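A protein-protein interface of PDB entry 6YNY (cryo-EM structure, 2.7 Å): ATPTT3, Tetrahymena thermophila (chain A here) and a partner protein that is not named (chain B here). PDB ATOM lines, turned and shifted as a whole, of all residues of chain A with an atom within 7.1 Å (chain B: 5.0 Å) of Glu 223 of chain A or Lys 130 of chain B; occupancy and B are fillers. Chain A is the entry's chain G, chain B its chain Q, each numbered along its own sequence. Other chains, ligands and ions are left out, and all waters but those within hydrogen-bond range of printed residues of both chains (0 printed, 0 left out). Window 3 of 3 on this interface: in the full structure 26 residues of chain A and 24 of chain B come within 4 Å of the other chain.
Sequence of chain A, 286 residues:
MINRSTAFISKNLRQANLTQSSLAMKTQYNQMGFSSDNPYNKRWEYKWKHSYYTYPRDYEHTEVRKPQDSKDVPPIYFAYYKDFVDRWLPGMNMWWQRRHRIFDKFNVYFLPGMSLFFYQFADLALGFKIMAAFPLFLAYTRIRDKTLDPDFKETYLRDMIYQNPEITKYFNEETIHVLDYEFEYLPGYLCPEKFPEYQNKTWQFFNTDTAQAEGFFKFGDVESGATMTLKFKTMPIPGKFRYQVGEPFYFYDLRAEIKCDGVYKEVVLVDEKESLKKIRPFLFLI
Lys 130 of chain B touches Val 222 of chain A (O to O, 3.6 Å).
Val 222 of chain A touches His 131 of chain B (CG2 to CG, 3.4 Å).
Glu 223 of chain A touches His 131 of chain B.
N of Gly 225 of chain A touches ND2 of Asn 134 of chain B, at 3.9 Å.
Hydrophobic or aromatic side chains of chain A within 4 Å of the printed part of chain B: Val 222.
Along chain A the printed residues that touch a printed residue of chain B span positions 222 to 225.
Printed residues of chain B that touch a printed residue of chain A: Lys 128, Lys 130, His 131 and Asn 134.
Hydrophobic or aromatic side chains of chain B within 4 Å of the printed part of chain A: His 131.
Among the printed residues, Asp or Glu carboxylates within 4 Å of a Lys or Arg side-chain nitrogen of the other chain: Glu 223 of chain A with Lys 128 of chain B (3.9 Å) and Glu 223 of chain A with Lys 130 of chain B (2.6 Å).
Glu 223 of chain A touches four residues of chain B.
Of chain A, only Val 222 (3.6 Å) and Glu 223 (2.6 Å) come within 4 Å of Lys 130 of chain B.
Of the printed residues of chain B, Gly 225 of chain A touches Asn 134.
Of the printed residues of chain B, Val 222 of chain A touches Lys 130, His 131 and Asn 134.
Printed residues of chain A within 4 Å of Lys 128 of chain B: Glu 223.
Printed residues of chain A within 4 Å of Asn 134 of chain B: Val 222 (2.8 Å), Glu 223 (3.4 Å) and Gly 225 (3.9 Å).
Of the printed residues of chain A, His 131 of chain B touches Val 222 and Glu 223.
Gly 220 of chain A touches none of the printed residues of chain B.
Tyr 170 of chain A touches none of the printed residues of chain B.
The nearest printed residue of chain B that does not touch Glu 223 of chain A is Asn 90 of chain B (6.3 Å).
The nearest residue of chain A that does not touch Lys 130 of chain B is Ser 224 of chain A (5.9 Å).
The backbone carbonyl oxygen (O) of Thr 175 of chain A sits at hydrogen-bond distance from the backbone NH (N) of Val 222 of chain A, 2.9 Å away.
N of Lys 128 of chain B sits at hydrogen-bond distance from ND1 of His 131 of chain B (3.3 Å).
The backbone carbonyl oxygen (O) of Lys 130 of chain B lies within hydrogen-bond range of the side-chain amide nitrogen (ND2) of Asn 134 of chain B (3.4 Å).
The backbone carbonyl oxygen (O) of Ile 89 of chain B is in hydrogen-bond range of the backbone NH (N) of Lys 130 of chain B (3.2 Å).
The side-chain carboxylate (OD2) of Asp 221 of chain A sits close to the backbone NH (N) of Glu 223 of chain A (3.4 Å).
ND2 of Asn 134 of chain B is in hydrogen-bond range of O of Val 222 of chain A, at 2.8 Å.
The side-chain amino group (NZ) of Lys 130 of chain B is in salt-bridge range of the side-chain carboxylate (OE2) of Glu 223 of chain A, at 2.6 Å.
The backbone carbonyl oxygen of Glu 223 of chain A is in hydrogen-bond range of the side-chain amide nitrogen of Asn 134 of chain B, at 3.4 Å.
NZ of Lys 128 of chain B is in salt-bridge range of OE2 of Glu 223 of chain A (3.9 Å).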
ATOM      1  N   TYR A 170     -22.090   1.330 -19.045  1.00  0.00           N
ATOM      2  CA  TYR A 170     -22.751   1.552 -20.319  1.00  0.00           C
ATOM      3  C   TYR A 170     -21.828   1.416 -21.518  1.00  0.00           C
ATOM      4  O   TYR A 170     -22.326   1.337 -22.647  1.00  0.00           O
ATOM      5  CB  TYR A 170     -23.388   2.949 -20.352  1.00  0.00           C
ATOM      6  CG  TYR A 170     -24.343   3.219 -19.217  1.00  0.00           C
ATOM      7  CD1 TYR A 170     -25.585   2.604 -19.168  1.00  0.00           C
ATOM      8  CD2 TYR A 170     -24.007   4.096 -18.198  1.00  0.00           C
ATOM      9  CE1 TYR A 170     -26.460   2.848 -18.134  1.00  0.00           C
ATOM     10  CE2 TYR A 170     -24.878   4.348 -17.159  1.00  0.00           C
ATOM     11  CZ  TYR A 170     -26.104   3.722 -17.132  1.00  0.00           C
ATOM     12  OH  TYR A 170     -26.976   3.970 -16.100  1.00  0.00           O
ATOM     13  N   ASN A 172     -18.196  -0.397 -23.325  1.00  0.00           N
ATOM     14  CA  ASN A 172     -17.167  -1.420 -23.348  1.00  0.00           C
ATOM     15  C   ASN A 172     -16.426  -1.323 -24.672  1.00  0.00           C
ATOM     16  O   ASN A 172     -17.001  -0.944 -25.695  1.00  0.00           O
ATOM     17  CB  ASN A 172     -17.756  -2.821 -23.163  1.00  0.00           C
ATOM     18  CG  ASN A 172     -16.698  -3.900 -23.139  1.00  0.00           C
ATOM     19  OD1 ASN A 172     -16.411  -4.529 -24.157  1.00  0.00           O
ATOM     20  ND2 ASN A 172     -16.106  -4.119 -21.973  1.00  0.00           N
ATOM     21  N   THR A 175     -17.785  -2.776 -27.803  1.00  0.00           N
ATOM     22  CA  THR A 175     -19.082  -2.287 -28.247  1.00  0.00           C
ATOM     23  C   THR A 175     -19.115  -0.773 -28.412  1.00  0.00           C
ATOM     24  O   THR A 175     -20.197  -0.215 -28.629  1.00  0.00           O
ATOM     25  CB  THR A 175     -20.174  -2.711 -27.262  1.00  0.00           C
ATOM     26  OG1 THR A 175     -19.868  -2.209 -25.957  1.00  0.00           O
ATOM     27  CG2 THR A 175     -20.277  -4.217 -27.204  1.00  0.00           C
ATOM     28  N   ILE A 176     -17.980  -0.098 -28.325  1.00  0.00           N
ATOM     29  CA  ILE A 176     -17.916   1.355 -28.403  1.00  0.00           C
ATOM     30  C   ILE A 176     -17.519   1.765 -29.812  1.00  0.00           C
ATOM     31  O   ILE A 176     -16.761   1.069 -30.497  1.00  0.00           O
ATOM     32  CB  ILE A 176     -16.927   1.916 -27.362  1.00  0.00           C
ATOM     33  CG1 ILE A 176     -17.058   3.428 -27.260  1.00  0.00           C
ATOM     34  CG2 ILE A 176     -15.513   1.567 -27.734  1.00  0.00           C
ATOM     35  CD1 ILE A 176     -16.183   4.022 -26.204  1.00  0.00           C
ATOM     36  N   HIS A 177     -18.033   2.911 -30.251  1.00  0.00           N
ATOM     37  CA  HIS A 177     -17.696   3.455 -31.555  1.00  0.00           C
ATOM     38  C   HIS A 177     -17.651   4.973 -31.473  1.00  0.00           C
ATOM     39  O   HIS A 177     -18.354   5.591 -30.671  1.00  0.00           O
ATOM     40  CB  HIS A 177     -18.691   3.010 -32.634  1.00  0.00           C
ATOM     41  CG  HIS A 177     -20.090   3.487 -32.411  1.00  0.00           C
ATOM     42  ND1 HIS A 177     -20.597   4.613 -33.022  1.00  0.00           N
ATOM     43  CD2 HIS A 177     -21.095   2.986 -31.656  1.00  0.00           C
ATOM     44  CE1 HIS A 177     -21.851   4.788 -32.648  1.00  0.00           C
ATOM     45  NE2 HIS A 177     -22.177   3.815 -31.819  1.00  0.00           N
ATOM     46  N   GLY A 220     -20.380   6.188 -28.641  1.00  0.00           N
ATOM     47  CA  GLY A 220     -21.635   5.459 -28.669  1.00  0.00           C
ATOM     48  C   GLY A 220     -21.385   3.993 -28.414  1.00  0.00           C
ATOM     49  O   GLY A 220     -20.347   3.447 -28.798  1.00  0.00           O
ATOM     50  N   ASP A 221     -22.343   3.352 -27.752  1.00  0.00           N
ATOM     51  CA  ASP A 221     -22.260   1.939 -27.413  1.00  0.00           C
ATOM     52  C   ASP A 221     -23.376   1.198 -28.132  1.00  0.00           C
ATOM     53  O   ASP A 221     -24.558   1.467 -27.898  1.00  0.00           O
ATOM     54  CB  ASP A 221     -22.354   1.726 -25.904  1.00  0.00           C
ATOM     55  CG  ASP A 221     -22.095   0.289 -25.504  1.00  0.00           C
ATOM     56  OD1 ASP A 221     -20.951  -0.178 -25.676  1.00  0.00           O
ATOM     57  OD2 ASP A 221     -23.034  -0.374 -25.019  1.00  0.00           O
ATOM     58  N   VAL A 222     -22.996   0.261 -29.003  1.00  0.00           N
ATOM     59  CA  VAL A 222     -23.969  -0.465 -29.806  1.00  0.00           C
ATOM     60  C   VAL A 222     -24.772  -1.474 -29.004  1.00  0.00           C
ATOM     61  O   VAL A 222     -25.760  -2.009 -29.518  1.00  0.00           O
ATOM     62  CB  VAL A 222     -23.264  -1.177 -30.980  1.00  0.00           C
ATOM     63  CG1 VAL A 222     -22.584  -0.168 -31.873  1.00  0.00           C
ATOM     64  CG2 VAL A 222     -22.255  -2.196 -30.474  1.00  0.00           C
ATOM     65  N   GLU A 223     -24.382  -1.749 -27.761  1.00  0.00           N
ATOM     66  CA  GLU A 223     -25.104  -2.704 -26.927  1.00  0.00           C
ATOM     67  C   GLU A 223     -26.159  -2.008 -26.072  1.00  0.00           C
ATOM     68  O   GLU A 223     -27.349  -2.319 -26.164  1.00  0.00           O
ATOM     69  CB  GLU A 223     -24.121  -3.471 -26.041  1.00  0.00           C
ATOM     70  CG  GLU A 223     -24.343  -4.971 -26.020  1.00  0.00           C
ATOM     71  CD  GLU A 223     -25.701  -5.359 -25.474  1.00  0.00           C
ATOM     72  OE1 GLU A 223     -26.305  -4.547 -24.744  1.00  0.00           O
ATOM     73  OE2 GLU A 223     -26.168  -6.477 -25.781  1.00  0.00           O
ATOM     74  N   SER A 224     -25.729  -1.066 -25.238  1.00  0.00           N
ATOM     75  CA  SER A 224     -26.635  -0.326 -24.372  1.00  0.00           C
ATOM     76  C   SER A 224     -27.304   0.850 -25.067  1.00  0.00           C
ATOM     77  O   SER A 224     -28.258   1.408 -24.518  1.00  0.00           O
ATOM     78  CB  SER A 224     -25.876   0.183 -23.149  1.00  0.00           C
ATOM     79  OG  SER A 224     -24.827   1.052 -23.534  1.00  0.00           O
ATOM     80  N   GLY A 225     -26.837   1.239 -26.250  1.00  0.00           N
ATOM     81  CA  GLY A 225     -27.388   2.399 -26.912  1.00  0.00           C
ATOM     82  C   GLY A 225     -27.043   3.711 -26.258  1.00  0.00           C
ATOM     83  O   GLY A 225     -27.672   4.727 -26.565  1.00  0.00           O
ATOM     84  N   ALA A 226     -26.061   3.721 -25.365  1.00  0.00           N
ATOM     85  CA  ALA A 226     -25.699   4.926 -24.642  1.00  0.00           C
ATOM     86  C   ALA A 226     -24.772   5.800 -25.470  1.00  0.00           C
ATOM     87  O   ALA A 226     -24.045   5.326 -26.347  1.00  0.00           O
ATOM     88  CB  ALA A 226     -25.028   4.568 -23.319  1.00  0.00           C
ATOM     89  N   ILE B  89     -33.843 -10.005 -32.997  1.00  0.00           N
ATOM     90  CA  ILE B  89     -33.135  -8.806 -32.570  1.00  0.00           C
ATOM     91  C   ILE B  89     -31.924  -9.161 -31.718  1.00  0.00           C
ATOM     92  O   ILE B  89     -30.902  -8.465 -31.761  1.00  0.00           O
ATOM     93  CB  ILE B  89     -34.100  -7.873 -31.815  1.00  0.00           C
ATOM     94  CG1 ILE B  89     -33.384  -6.607 -31.350  1.00  0.00           C
ATOM     95  CG2 ILE B  89     -34.713  -8.588 -30.622  1.00  0.00           C
ATOM     96  CD1 ILE B  89     -32.796  -5.806 -32.463  1.00  0.00           C
ATOM     97  N   ASN B  90     -32.006 -10.237 -30.940  1.00  0.00           N
ATOM     98  CA  ASN B  90     -30.948 -10.636 -30.017  1.00  0.00           C
ATOM     99  C   ASN B  90     -30.129 -11.797 -30.561  1.00  0.00           C
ATOM    100  O   ASN B  90     -29.684 -12.663 -29.804  1.00  0.00           O
ATOM    101  CB  ASN B  90     -31.547 -11.002 -28.664  1.00  0.00           C
ATOM    102  CG  ASN B  90     -32.347  -9.873 -28.057  1.00  0.00           C
ATOM    103  OD1 ASN B  90     -33.564  -9.971 -27.904  1.00  0.00           O
ATOM    104  ND2 ASN B  90     -31.668  -8.794 -27.696  1.00  0.00           N
ATOM    105  N   LYS B 128     -23.691  -8.096 -33.710  1.00  0.00           N
ATOM    106  CA  LYS B 128     -25.038  -8.558 -33.424  1.00  0.00           C
ATOM    107  C   LYS B 128     -26.033  -7.724 -34.211  1.00  0.00           C
ATOM    108  O   LYS B 128     -25.729  -6.622 -34.671  1.00  0.00           O
ATOM    109  CB  LYS B 128     -25.369  -8.472 -31.932  1.00  0.00           C
ATOM    110  CG  LYS B 128     -24.481  -9.304 -31.046  1.00  0.00           C
ATOM    111  CD  LYS B 128     -24.873  -9.147 -29.594  1.00  0.00           C
ATOM    112  CE  LYS B 128     -23.911  -9.869 -28.672  1.00  0.00           C
ATOM    113  NZ  LYS B 128     -24.181  -9.558 -27.244  1.00  0.00           N
ATOM    114  N   VAL B 129     -27.238  -8.271 -34.360  1.00  0.00           N
ATOM    115  CA  VAL B 129     -28.319  -7.523 -34.991  1.00  0.00           C
ATOM    116  C   VAL B 129     -28.655  -6.295 -34.161  1.00  0.00           C
ATOM    117  O   VAL B 129     -28.926  -5.215 -34.698  1.00  0.00           O
ATOM    118  CB  VAL B 129     -29.547  -8.429 -35.183  1.00  0.00           C
ATOM    119  CG1 VAL B 129     -30.693  -7.652 -35.774  1.00  0.00           C
ATOM    120  CG2 VAL B 129     -29.198  -9.602 -36.063  1.00  0.00           C
ATOM    121  N   LYS B 130     -28.640  -6.443 -32.837  1.00  0.00           N
ATOM    122  CA  LYS B 130     -28.914  -5.315 -31.956  1.00  0.00           C
ATOM    123  C   LYS B 130     -27.905  -4.194 -32.153  1.00  0.00           C
ATOM    124  O   LYS B 130     -28.223  -3.024 -31.917  1.00  0.00           O
ATOM    125  CB  LYS B 130     -28.899  -5.792 -30.507  1.00  0.00           C
ATOM    126  CG  LYS B 130     -29.442  -4.807 -29.506  1.00  0.00           C
ATOM    127  CD  LYS B 130     -28.913  -5.113 -28.115  1.00  0.00           C
ATOM    128  CE  LYS B 130     -29.252  -6.527 -27.681  1.00  0.00           C
ATOM    129  NZ  LYS B 130     -28.672  -6.843 -26.352  1.00  0.00           N
ATOM    130  N   HIS B 131     -26.688  -4.530 -32.582  1.00  0.00           N
ATOM    131  CA  HIS B 131     -25.659  -3.512 -32.756  1.00  0.00           C
ATOM    132  C   HIS B 131     -25.928  -2.660 -33.986  1.00  0.00           C
ATOM    133  O   HIS B 131     -25.737  -1.439 -33.956  1.00  0.00           O
ATOM    134  CB  HIS B 131     -24.286  -4.170 -32.851  1.00  0.00           C
ATOM    135  CG  HIS B 131     -23.899  -4.935 -31.626  1.00  0.00           C
ATOM    136  ND1 HIS B 131     -22.767  -5.719 -31.567  1.00  0.00           N
ATOM    137  CD2 HIS B 131     -24.487  -5.030 -30.412  1.00  0.00           C
ATOM    138  CE1 HIS B 131     -22.679  -6.268 -30.369  1.00  0.00           C
ATOM    139  NE2 HIS B 131     -23.709  -5.865 -29.649  1.00  0.00           N
ATOM    140  N   PHE B 132     -26.360  -3.284 -35.081  1.00  0.00           N
ATOM    141  CA  PHE B 132     -26.682  -2.527 -36.283  1.00  0.00           C
ATOM    142  C   PHE B 132     -27.854  -1.587 -36.050  1.00  0.00           C
ATOM    143  O   PHE B 132     -27.919  -0.513 -36.656  1.00  0.00           O
ATOM    144  CB  PHE B 132     -26.995  -3.478 -37.433  1.00  0.00           C
ATOM    145  CG  PHE B 132     -25.787  -4.133 -38.024  1.00  0.00           C
ATOM    146  CD1 PHE B 132     -25.160  -3.583 -39.122  1.00  0.00           C
ATOM    147  CD2 PHE B 132     -25.282  -5.300 -37.488  1.00  0.00           C
ATOM    148  CE1 PHE B 132     -24.052  -4.181 -39.671  1.00  0.00           C
ATOM    149  CE2 PHE B 132     -24.175  -5.901 -38.033  1.00  0.00           C
ATOM    150  CZ  PHE B 132     -23.559  -5.342 -39.125  1.00  0.00           C
ATOM    151  N   VAL B 133     -28.785  -1.974 -35.180  1.00  0.00           N
ATOM    152  CA  VAL B 133     -29.954  -1.142 -34.919  1.00  0.00           C
ATOM    153  C   VAL B 133     -29.560   0.097 -34.129  1.00  0.00           C
ATOM    154  O   VAL B 133     -29.941   1.220 -34.474  1.00  0.00           O
ATOM    155  CB  VAL B 133     -31.029  -1.959 -34.185  1.00  0.00           C
ATOM    156  CG1 VAL B 133     -32.202  -1.080 -33.813  1.00  0.00           C
ATOM    157  CG2 VAL B 133     -31.481  -3.117 -35.041  1.00  0.00           C
ATOM    158  N   ASN B 134     -28.791  -0.087 -33.057  1.00  0.00           N
ATOM    159  CA  ASN B 134     -28.413   1.047 -32.225  1.00  0.00           C
ATOM    160  C   ASN B 134     -27.449   1.977 -32.944  1.00  0.00           C
ATOM    161  O   ASN B 134     -27.506   3.196 -32.748  1.00  0.00           O
ATOM    162  CB  ASN B 134     -27.806   0.558 -30.916  1.00  0.00           C
ATOM    163  CG  ASN B 134     -28.821  -0.102 -30.016  1.00  0.00           C
ATOM    164  OD1 ASN B 134     -30.015   0.177 -30.098  1.00  0.00           O
ATOM    165  ND2 ASN B 134     -28.349  -0.978 -29.143  1.00  0.00           N
